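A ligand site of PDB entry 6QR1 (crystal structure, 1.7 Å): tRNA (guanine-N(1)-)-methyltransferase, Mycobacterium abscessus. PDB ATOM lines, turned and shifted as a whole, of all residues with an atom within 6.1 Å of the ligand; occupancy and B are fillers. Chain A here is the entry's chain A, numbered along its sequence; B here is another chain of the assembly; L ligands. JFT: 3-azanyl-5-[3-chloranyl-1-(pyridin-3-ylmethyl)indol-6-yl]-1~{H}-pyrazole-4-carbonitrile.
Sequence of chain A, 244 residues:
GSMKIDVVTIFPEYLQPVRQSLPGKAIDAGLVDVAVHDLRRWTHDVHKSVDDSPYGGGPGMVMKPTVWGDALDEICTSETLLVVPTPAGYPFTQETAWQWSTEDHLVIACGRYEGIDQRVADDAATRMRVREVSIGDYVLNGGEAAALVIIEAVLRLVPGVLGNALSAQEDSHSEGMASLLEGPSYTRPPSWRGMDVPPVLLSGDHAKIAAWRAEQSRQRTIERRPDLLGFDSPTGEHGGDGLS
The backbone carbonyl oxygen of Gly 115 is in hydrogen-bond range of the backbone NH of Met 63 (2.8 Å). NE of Arg 156 of chain B sits at hydrogen-bond distance from OD1 of Asn 141 (3.0 Å). OG of Ser 134 sits at hydrogen-bond distance from O of Gly 136 (3.0 Å). O of Gly 111 is in hydrogen-bond range of N of Gly 143. The side-chain hydroxyl of Tyr 138 lies within hydrogen-bond range of the backbone carbonyl oxygen of Ile 135. N of Arg 112 is in hydrogen-bond range of SD of Met 63 (3.3 Å). The backbone NH (N) of Val 133 is in hydrogen-bond range of the backbone carbonyl oxygen (O) of Val 84 (3.1 Å). The backbone carbonyl oxygen (O) of Val 133 is in hydrogen-bond range of the backbone NH (N) of Thr 86 (2.9 Å).
N19 of the ligand sits at hydrogen-bond distance from OG of Ser 134 (3.1 Å). N of Leu 140 is in hydrogen-bond range of N17 of the ligand. N of Thr 86 is in hydrogen-bond range of N22 of the ligand, 3.5 Å away. N19 of the ligand lies within hydrogen-bond range of O of Gly 136 (3.0 Å). O of Tyr 138 sits close to N19 of the ligand.
A nitrogen (N04) of the ligand sits close to the backbone carbonyl oxygen (O) of Tyr 113 (3.5 Å). A nitrogen (N22) of the ligand sits close to the backbone carbonyl oxygen of Val 133, at 3.3 Å. Residues that only touch the ligand: Pro 85 (3.1 Å), Gly 111 (3.1 Å), Asn 141 (3.3 Å), Pro 87 (3.4 Å), Ala 146 (3.5 Å), Val 139 (3.5 Å), Ile 135 (3.5 Å), Arg 112 (3.5 Å), Gly 142 (3.6 Å), Glu 114 (3.6 Å), Gly 143 (3.8 Å), Gly 115 (3.8 Å) and Glu 182 of chain B (3.96 Å). Hydrophobic or aromatic side chains that line the ligand: Pro 85, Pro 87, Ile 135, Tyr 138, Val 139, Leu 140 and Ala 146. Of the 28 residues printed, 20 come within 4 Å of the ligand.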
ATOM      1  N   MET A  63     -13.224  19.635 -26.562  1.00  0.00           N
ATOM      2  CA  MET A  63     -11.874  19.104 -26.480  1.00  0.00           C
ATOM      3  C   MET A  63     -11.848  17.595 -26.612  1.00  0.00           C
ATOM      4  O   MET A  63     -12.708  16.881 -26.087  1.00  0.00           O
ATOM      5  CB  MET A  63     -11.196  19.557 -25.194  1.00  0.00           C
ATOM      6  CG  MET A  63     -11.182  21.073 -25.075  1.00  0.00           C
ATOM      7  SD  MET A  63      -9.949  21.627 -23.868  1.00  0.00           S
ATOM      8  CE  MET A  63      -8.511  21.908 -24.879  1.00  0.00           C
ATOM      9  N   VAL A  84     -11.946  19.318 -12.151  1.00  0.00           N
ATOM     10  CA  VAL A  84     -12.269  19.773 -13.501  1.00  0.00           C
ATOM     11  C   VAL A  84     -13.167  20.983 -13.401  1.00  0.00           C
ATOM     12  O   VAL A  84     -14.366  20.853 -13.153  1.00  0.00           O
ATOM     13  CB  VAL A  84     -12.986  18.686 -14.328  1.00  0.00           C
ATOM     14  CG1 VAL A  84     -13.163  19.195 -15.748  1.00  0.00           C
ATOM     15  CG2 VAL A  84     -12.187  17.381 -14.338  1.00  0.00           C
ATOM     16  N   PRO A  85     -12.586  22.182 -13.565  1.00  0.00           N
ATOM     17  CA  PRO A  85     -13.428  23.375 -13.571  1.00  0.00           C
ATOM     18  C   PRO A  85     -14.421  23.304 -14.720  1.00  0.00           C
ATOM     19  O   PRO A  85     -14.086  22.856 -15.831  1.00  0.00           O
ATOM     20  CB  PRO A  85     -12.425  24.520 -13.748  1.00  0.00           C
ATOM     21  CG  PRO A  85     -11.120  23.971 -13.164  1.00  0.00           C
ATOM     22  CD  PRO A  85     -11.143  22.507 -13.570  1.00  0.00           C
ATOM     23  N   THR A  86     -15.656  23.709 -14.442  1.00  0.00           N
ATOM     24  CA  THR A  86     -16.709  23.766 -15.453  1.00  0.00           C
ATOM     25  C   THR A  86     -17.863  24.620 -14.946  1.00  0.00           C
ATOM     26  O   THR A  86     -18.192  24.573 -13.773  1.00  0.00           O
ATOM     27  CB  THR A  86     -17.228  22.359 -15.858  1.00  0.00           C
ATOM     28  OG1 THR A  86     -18.470  22.466 -16.563  1.00  0.00           O
ATOM     29  CG2 THR A  86     -17.378  21.443 -14.671  1.00  0.00           C
ATOM     30  N   PRO A  87     -18.461  25.430 -15.829  1.00  0.00           N
ATOM     31  CA  PRO A  87     -19.590  26.240 -15.391  1.00  0.00           C
ATOM     32  C   PRO A  87     -20.767  25.366 -14.958  1.00  0.00           C
ATOM     33  O   PRO A  87     -21.656  25.845 -14.264  1.00  0.00           O
ATOM     34  CB  PRO A  87     -19.924  27.087 -16.626  1.00  0.00           C
ATOM     35  CG  PRO A  87     -19.384  26.318 -17.775  1.00  0.00           C
ATOM     36  CD  PRO A  87     -18.219  25.519 -17.284  1.00  0.00           C
ATOM     37  N   ALA A 109      -7.630  19.916 -14.421  1.00  0.00           N
ATOM     38  CA  ALA A 109      -7.751  19.810 -15.867  1.00  0.00           C
ATOM     39  C   ALA A 109      -8.515  21.000 -16.410  1.00  0.00           C
ATOM     40  O   ALA A 109      -9.740  21.071 -16.285  1.00  0.00           O
ATOM     41  CB  ALA A 109      -8.475  18.512 -16.248  1.00  0.00           C
ATOM     42  N   CYS A 110      -7.786  21.922 -17.030  1.00  0.00           N
ATOM     43  CA  CYS A 110      -8.359  23.161 -17.552  1.00  0.00           C
ATOM     44  C   CYS A 110      -8.734  23.020 -19.005  1.00  0.00           C
ATOM     45  O   CYS A 110      -7.846  22.832 -19.859  1.00  0.00           O
ATOM     46  CB  CYS A 110      -7.370  24.314 -17.421  1.00  0.00           C
ATOM     47  SG  CYS A 110      -6.862  24.679 -15.742  1.00  0.00           S
ATOM     48  N   GLY A 111     -10.017  23.141 -19.307  1.00  0.00           N
ATOM     49  CA  GLY A 111     -10.456  23.094 -20.683  1.00  0.00           C
ATOM     50  C   GLY A 111     -10.781  24.457 -21.266  1.00  0.00           C
ATOM     51  O   GLY A 111     -10.685  25.489 -20.586  1.00  0.00           O
ATOM     52  N   ARG A 112     -11.168  24.437 -22.535  1.00  0.00           N
ATOM     53  CA  ARG A 112     -11.539  25.629 -23.285  1.00  0.00           C
ATOM     54  C   ARG A 112     -12.696  25.275 -24.203  1.00  0.00           C
ATOM     55  O   ARG A 112     -13.187  24.139 -24.177  1.00  0.00           O
ATOM     56  CB  ARG A 112     -10.358  26.167 -24.093  1.00  0.00           C
ATOM     57  CG  ARG A 112      -9.287  26.891 -23.275  1.00  0.00           C
ATOM     58  CD  ARG A 112      -9.494  28.397 -23.323  1.00  0.00           C
ATOM     59  NE  ARG A 112      -9.008  29.038 -22.111  1.00  0.00           N
ATOM     60  CZ  ARG A 112      -8.958  30.351 -21.927  1.00  0.00           C
ATOM     61  NH1 ARG A 112      -9.357  31.178 -22.884  1.00  0.00           N
ATOM     62  NH2 ARG A 112      -8.500  30.834 -20.766  1.00  0.00           N
ATOM     63  N   TYR A 113     -13.127  26.233 -25.025  1.00  0.00           N
ATOM     64  CA  TYR A 113     -14.233  26.039 -25.962  1.00  0.00           C
ATOM     65  C   TYR A 113     -15.492  25.627 -25.205  1.00  0.00           C
ATOM     66  O   TYR A 113     -15.791  26.191 -24.154  1.00  0.00           O
ATOM     67  CB  TYR A 113     -13.844  25.007 -27.017  1.00  0.00           C
ATOM     68  CG  TYR A 113     -12.455  25.276 -27.569  1.00  0.00           C
ATOM     69  CD1 TYR A 113     -12.183  26.475 -28.219  1.00  0.00           C
ATOM     70  CD2 TYR A 113     -11.434  24.363 -27.417  1.00  0.00           C
ATOM     71  CE1 TYR A 113     -10.924  26.736 -28.714  1.00  0.00           C
ATOM     72  CE2 TYR A 113     -10.167  24.613 -27.906  1.00  0.00           C
ATOM     73  CZ  TYR A 113      -9.917  25.809 -28.566  1.00  0.00           C
ATOM     74  OH  TYR A 113      -8.665  26.076 -29.057  1.00  0.00           O
ATOM     75  N   GLU A 114     -16.237  24.642 -25.711  1.00  0.00           N
ATOM     76  CA  GLU A 114     -17.486  24.301 -25.021  1.00  0.00           C
ATOM     77  C   GLU A 114     -17.307  23.295 -23.888  1.00  0.00           C
ATOM     78  O   GLU A 114     -18.249  22.987 -23.166  1.00  0.00           O
ATOM     79  CB  GLU A 114     -18.505  23.786 -26.036  1.00  0.00           C
ATOM     80  CG  GLU A 114     -18.534  24.607 -27.312  1.00  0.00           C
ATOM     81  CD  GLU A 114     -18.781  26.083 -27.044  1.00  0.00           C
ATOM     82  OE1 GLU A 114     -19.884  26.424 -26.546  1.00  0.00           O
ATOM     83  OE2 GLU A 114     -17.875  26.903 -27.300  1.00  0.00           O
ATOM     84  N   GLY A 115     -16.084  22.793 -23.696  1.00  0.00           N
ATOM     85  CA  GLY A 115     -15.859  21.817 -22.655  1.00  0.00           C
ATOM     86  C   GLY A 115     -15.013  20.656 -23.116  1.00  0.00           C
ATOM     87  O   GLY A 115     -14.562  20.630 -24.261  1.00  0.00           O
ATOM     88  N   ILE A 116     -14.761  19.731 -22.210  1.00  0.00           N
ATOM     89  CA  ILE A 116     -14.000  18.503 -22.490  1.00  0.00           C
ATOM     90  C   ILE A 116     -14.993  17.376 -22.720  1.00  0.00           C
ATOM     91  O   ILE A 116     -15.956  17.274 -21.985  1.00  0.00           O
ATOM     92  CB  ILE A 116     -13.062  18.160 -21.334  1.00  0.00           C
ATOM     93  CG1 ILE A 116     -12.165  19.364 -21.010  1.00  0.00           C
ATOM     94  CG2 ILE A 116     -12.249  16.887 -21.633  1.00  0.00           C
ATOM     95  CD1 ILE A 116     -11.302  19.155 -19.779  1.00  0.00           C
ATOM     96  N   VAL A 133     -16.312  21.177 -10.786  1.00  0.00           N
ATOM     97  CA  VAL A 133     -16.710  22.284  -9.917  1.00  0.00           C
ATOM     98  C   VAL A 133     -16.731  23.599 -10.641  1.00  0.00           C
ATOM     99  O   VAL A 133     -15.997  23.808 -11.607  1.00  0.00           O
ATOM    100  CB  VAL A 133     -15.766  22.434  -8.690  1.00  0.00           C
ATOM    101  CG1 VAL A 133     -15.800  21.192  -7.811  1.00  0.00           C
ATOM    102  CG2 VAL A 133     -14.327  22.743  -9.128  1.00  0.00           C
ATOM    103  N   SER A 134     -17.576  24.496 -10.140  1.00  0.00           N
ATOM    104  CA  SER A 134     -17.645  25.879 -10.635  1.00  0.00           C
ATOM    105  C   SER A 134     -17.307  26.865  -9.527  1.00  0.00           C
ATOM    106  O   SER A 134     -17.743  26.691  -8.391  1.00  0.00           O
ATOM    107  CB  SER A 134     -19.035  26.180 -11.182  1.00  0.00           C
ATOM    108  OG  SER A 134     -19.174  27.572 -11.428  1.00  0.00           O
ATOM    109  N   ILE A 135     -16.559  27.912  -9.854  1.00  0.00           N
ATOM    110  CA  ILE A 135     -16.163  28.881  -8.819  1.00  0.00           C
ATOM    111  C   ILE A 135     -17.179  30.018  -8.672  1.00  0.00           C
ATOM    112  O   ILE A 135     -17.037  30.858  -7.790  1.00  0.00           O
ATOM    113  CB  ILE A 135     -14.773  29.487  -9.095  1.00  0.00           C
ATOM    114  CG1 ILE A 135     -14.716  30.166 -10.463  1.00  0.00           C
ATOM    115  CG2 ILE A 135     -13.689  28.405  -8.932  1.00  0.00           C
ATOM    116  CD1 ILE A 135     -13.591  31.251 -10.606  1.00  0.00           C
ATOM    117  N   GLY A 136     -18.218  30.024  -9.498  1.00  0.00           N
ATOM    118  CA  GLY A 136     -19.219  31.057  -9.348  1.00  0.00           C
ATOM    119  C   GLY A 136     -20.206  31.110 -10.493  1.00  0.00           C
ATOM    120  O   GLY A 136     -20.041  30.410 -11.482  1.00  0.00           O
ATOM    121  N   ASP A 137     -21.210  31.973 -10.348  1.00  0.00           N
ATOM    122  CA  ASP A 137     -22.289  32.032 -11.333  1.00  0.00           C
ATOM    123  C   ASP A 137     -22.037  33.076 -12.391  1.00  0.00           C
ATOM    124  O   ASP A 137     -22.766  34.071 -12.485  1.00  0.00           O
ATOM    125  CB  ASP A 137     -23.616  32.291 -10.633  1.00  0.00           C
ATOM    126  CG  ASP A 137     -24.073  31.101  -9.820  1.00  0.00           C
ATOM    127  OD1 ASP A 137     -23.705  29.977 -10.190  1.00  0.00           O
ATOM    128  OD2 ASP A 137     -24.791  31.298  -8.814  1.00  0.00           O
ATOM    129  N   TYR A 138     -20.996  32.843 -13.176  1.00  0.00           N
ATOM    130  CA  TYR A 138     -20.636  33.674 -14.307  1.00  0.00           C
ATOM    131  C   TYR A 138     -19.911  32.756 -15.272  1.00  0.00           C
ATOM    132  O   TYR A 138     -19.454  31.679 -14.880  1.00  0.00           O
ATOM    133  CB  TYR A 138     -19.722  34.846 -13.900  1.00  0.00           C
ATOM    134  CG  TYR A 138     -18.778  34.455 -12.790  1.00  0.00           C
ATOM    135  CD1 TYR A 138     -17.656  33.665 -13.061  1.00  0.00           C
ATOM    136  CD2 TYR A 138     -19.031  34.832 -11.467  1.00  0.00           C
ATOM    137  CE1 TYR A 138     -16.806  33.269 -12.043  1.00  0.00           C
ATOM    138  CE2 TYR A 138     -18.166  34.449 -10.443  1.00  0.00           C
ATOM    139  CZ  TYR A 138     -17.062  33.671 -10.740  1.00  0.00           C
ATOM    140  OH  TYR A 138     -16.227  33.278  -9.729  1.00  0.00           O
ATOM    141  N   VAL A 139     -19.775  33.206 -16.504  1.00  0.00           N
ATOM    142  CA  VAL A 139     -19.172  32.394 -17.547  1.00  0.00           C
ATOM    143  C   VAL A 139     -17.782  32.920 -17.884  1.00  0.00           C
ATOM    144  O   VAL A 139     -17.590  34.104 -18.106  1.00  0.00           O
ATOM    145  CB  VAL A 139     -20.038  32.385 -18.816  1.00  0.00           C
ATOM    146  CG1 VAL A 139     -19.416  31.485 -19.871  1.00  0.00           C
ATOM    147  CG2 VAL A 139     -21.456  31.949 -18.487  1.00  0.00           C
ATOM    148  N   LEU A 140     -16.813  32.004 -17.906  1.00  0.00           N
ATOM    149  CA  LEU A 140     -15.458  32.328 -18.315  1.00  0.00           C
ATOM    150  C   LEU A 140     -15.155  31.642 -19.650  1.00  0.00           C
ATOM    151  O   LEU A 140     -15.967  30.885 -20.159  1.00  0.00           O
ATOM    152  CB  LEU A 140     -14.463  31.870 -17.244  1.00  0.00           C
ATOM    153  CG  LEU A 140     -14.716  32.373 -15.826  1.00  0.00           C
ATOM    154  CD1 LEU A 140     -13.784  31.678 -14.851  1.00  0.00           C
ATOM    155  CD2 LEU A 140     -14.528  33.884 -15.765  1.00  0.00           C
ATOM    156  N   ASN A 141     -13.983  31.917 -20.227  1.00  0.00           N
ATOM    157  CA  ASN A 141     -13.659  31.295 -21.511  1.00  0.00           C
ATOM    158  C   ASN A 141     -13.079  29.899 -21.347  1.00  0.00           C
ATOM    159  O   ASN A 141     -13.033  29.117 -22.304  1.00  0.00           O
ATOM    160  CB  ASN A 141     -12.653  32.149 -22.267  1.00  0.00           C
ATOM    161  CG  ASN A 141     -13.267  33.389 -22.839  1.00  0.00           C
ATOM    162  OD1 ASN A 141     -14.394  33.355 -23.348  1.00  0.00           O
ATOM    163  ND2 ASN A 141     -12.556  34.498 -22.750  1.00  0.00           N
ATOM    164  N   GLY A 142     -12.617  29.592 -20.146  1.00  0.00           N
ATOM    165  CA  GLY A 142     -12.037  28.289 -19.913  1.00  0.00           C
ATOM    166  C   GLY A 142     -11.691  28.148 -18.448  1.00  0.00           C
ATOM    167  O   GLY A 142     -12.001  29.034 -17.653  1.00  0.00           O
ATOM    168  N   GLY A 143     -11.043  27.040 -18.096  1.00  0.00           N
ATOM    169  CA  GLY A 143     -10.838  26.701 -16.698  1.00  0.00           C
ATOM    170  C   GLY A 143      -9.663  27.382 -16.015  1.00  0.00           C
ATOM    171  O   GLY A 143      -9.525  27.261 -14.793  1.00  0.00           O
ATOM    172  N   ALA A 146     -10.309  29.827 -13.098  1.00  0.00           N
ATOM    173  CA  ALA A 146     -10.891  29.045 -12.015  1.00  0.00           C
ATOM    174  C   ALA A 146      -9.797  28.260 -11.284  1.00  0.00           C
ATOM    175  O   ALA A 146      -9.810  28.143 -10.064  1.00  0.00           O
ATOM    176  CB  ALA A 146     -11.962  28.103 -12.548  1.00  0.00           C
ATOM    177  N   ILE A 150      -8.941  28.314  -7.339  1.00  0.00           N
ATOM    178  CA  ILE A 150      -8.920  27.092  -6.548  1.00  0.00           C
ATOM    179  C   ILE A 150      -7.566  26.867  -5.869  1.00  0.00           C
ATOM    180  O   ILE A 150      -7.488  26.541  -4.683  1.00  0.00           O
ATOM    181  CB  ILE A 150      -9.291  25.881  -7.424  1.00  0.00           C
ATOM    182  CG1 ILE A 150     -10.745  26.005  -7.871  1.00  0.00           C
ATOM    183  CG2 ILE A 150      -9.047  24.567  -6.673  1.00  0.00           C
ATOM    184  CD1 ILE A 150     -11.118  25.067  -9.017  1.00  0.00           C
ATOM    185  N   ARG B 156     -15.375  39.117 -22.335  1.00  0.00           N
ATOM    186  CA  ARG B 156     -15.918  38.232 -23.356  1.00  0.00           C
ATOM    187  C   ARG B 156     -17.329  38.668 -23.779  1.00  0.00           C
ATOM    188  O   ARG B 156     -17.869  38.163 -24.772  1.00  0.00           O
ATOM    189  CB  ARG B 156     -15.917  36.789 -22.871  1.00  0.00           C
ATOM    190  CG  ARG B 156     -16.750  36.534 -21.623  1.00  0.00           C
ATOM    191  CD  ARG B 156     -16.585  35.088 -21.138  1.00  0.00           C
ATOM    192  NE  ARG B 156     -17.031  34.089 -22.114  1.00  0.00           N
ATOM    193  CZ  ARG B 156     -18.301  33.769 -22.319  1.00  0.00           C
ATOM    194  NH1 ARG B 156     -19.273  34.383 -21.648  1.00  0.00           N
ATOM    195  NH2 ARG B 156     -18.631  32.845 -23.217  1.00  0.00           N
ATOM    196  N   GLU B 182     -25.129  23.728 -18.337  1.00  0.00           N
ATOM    197  CA  GLU B 182     -24.754  23.053 -19.575  1.00  0.00           C
ATOM    198  C   GLU B 182     -24.705  21.550 -19.383  1.00  0.00           C
ATOM    199  O   GLU B 182     -24.178  21.063 -18.390  1.00  0.00           O
ATOM    200  CB  GLU B 182     -23.391  23.545 -20.072  1.00  0.00           C
ATOM    201  CG  GLU B 182     -23.270  25.043 -20.277  1.00  0.00           C
ATOM    202  CD  GLU B 182     -24.046  25.546 -21.477  1.00  0.00           C
ATOM    203  OE1 GLU B 182     -24.577  24.720 -22.247  1.00  0.00           O
ATOM    204  OE2 GLU B 182     -24.125  26.784 -21.660  1.00  0.00           O
HETATM  205  C13 JFT L   1     -15.739  27.783 -18.394  1.00  0.00           C
HETATM  206  C15 JFT L   1     -16.149  28.504 -16.044  1.00  0.00           C
HETATM  207  C20 JFT L   1     -16.294  28.393 -14.635  1.00  0.00           C
HETATM  208  C21 JFT L   1     -15.635  27.457 -13.652  1.00  0.00           C
HETATM  209  C24 JFT L   1     -14.435  25.447 -17.538  1.00  0.00           C
HETATM  210  C02 JFT L   1     -14.308  24.988 -20.117  1.00  0.00           C
HETATM  211  C03 JFT L   1     -14.759  25.737 -21.239  1.00  0.00           C
HETATM  212  C05 JFT L   1     -15.954  27.893 -21.526  1.00  0.00           C
HETATM  213  C06 JFT L   1     -17.460  27.622 -21.620  1.00  0.00           C
HETATM  214  C07 JFT L   1     -17.955  26.298 -21.629  1.00  0.00           C
HETATM  215  C08 JFT L   1     -19.352  26.103 -21.711  1.00  0.00           C
HETATM  216  C09 JFT L   1     -20.195  27.241 -21.766  1.00  0.00           C
HETATM  217  C11 JFT L   1     -18.383  28.682 -21.680  1.00  0.00           C
HETATM  218  C12 JFT L   1     -15.277  26.849 -19.356  1.00  0.00           C
HETATM  219  C14 JFT L   1     -15.502  27.553 -17.026  1.00  0.00           C
HETATM  220  C18 JFT L   1     -17.109  29.421 -14.254  1.00  0.00           C
HETATM  221  C23 JFT L   1     -14.904  26.361 -16.585  1.00  0.00           C
HETATM  222  C25 JFT L   1     -14.633  25.701 -18.922  1.00  0.00           C
HETATM  223  N04 JFT L   1     -15.342  26.844 -20.749  1.00  0.00           N
HETATM  224  N10 JFT L   1     -19.684  28.462 -21.753  1.00  0.00           N
HETATM  225  N16 JFT L   1     -16.978  29.492 -16.453  1.00  0.00           N
HETATM  226  N17 JFT L   1     -17.508  30.067 -15.355  1.00  0.00           N
HETATM  227  N19 JFT L   1     -17.487  29.730 -12.880  1.00  0.00           N
HETATM  228  N22 JFT L   1     -15.171  26.777 -12.879  1.00  0.00           N
HETATM  229 CL1  JFT L   1     -13.524  23.453 -20.091  1.00  0.00          CL
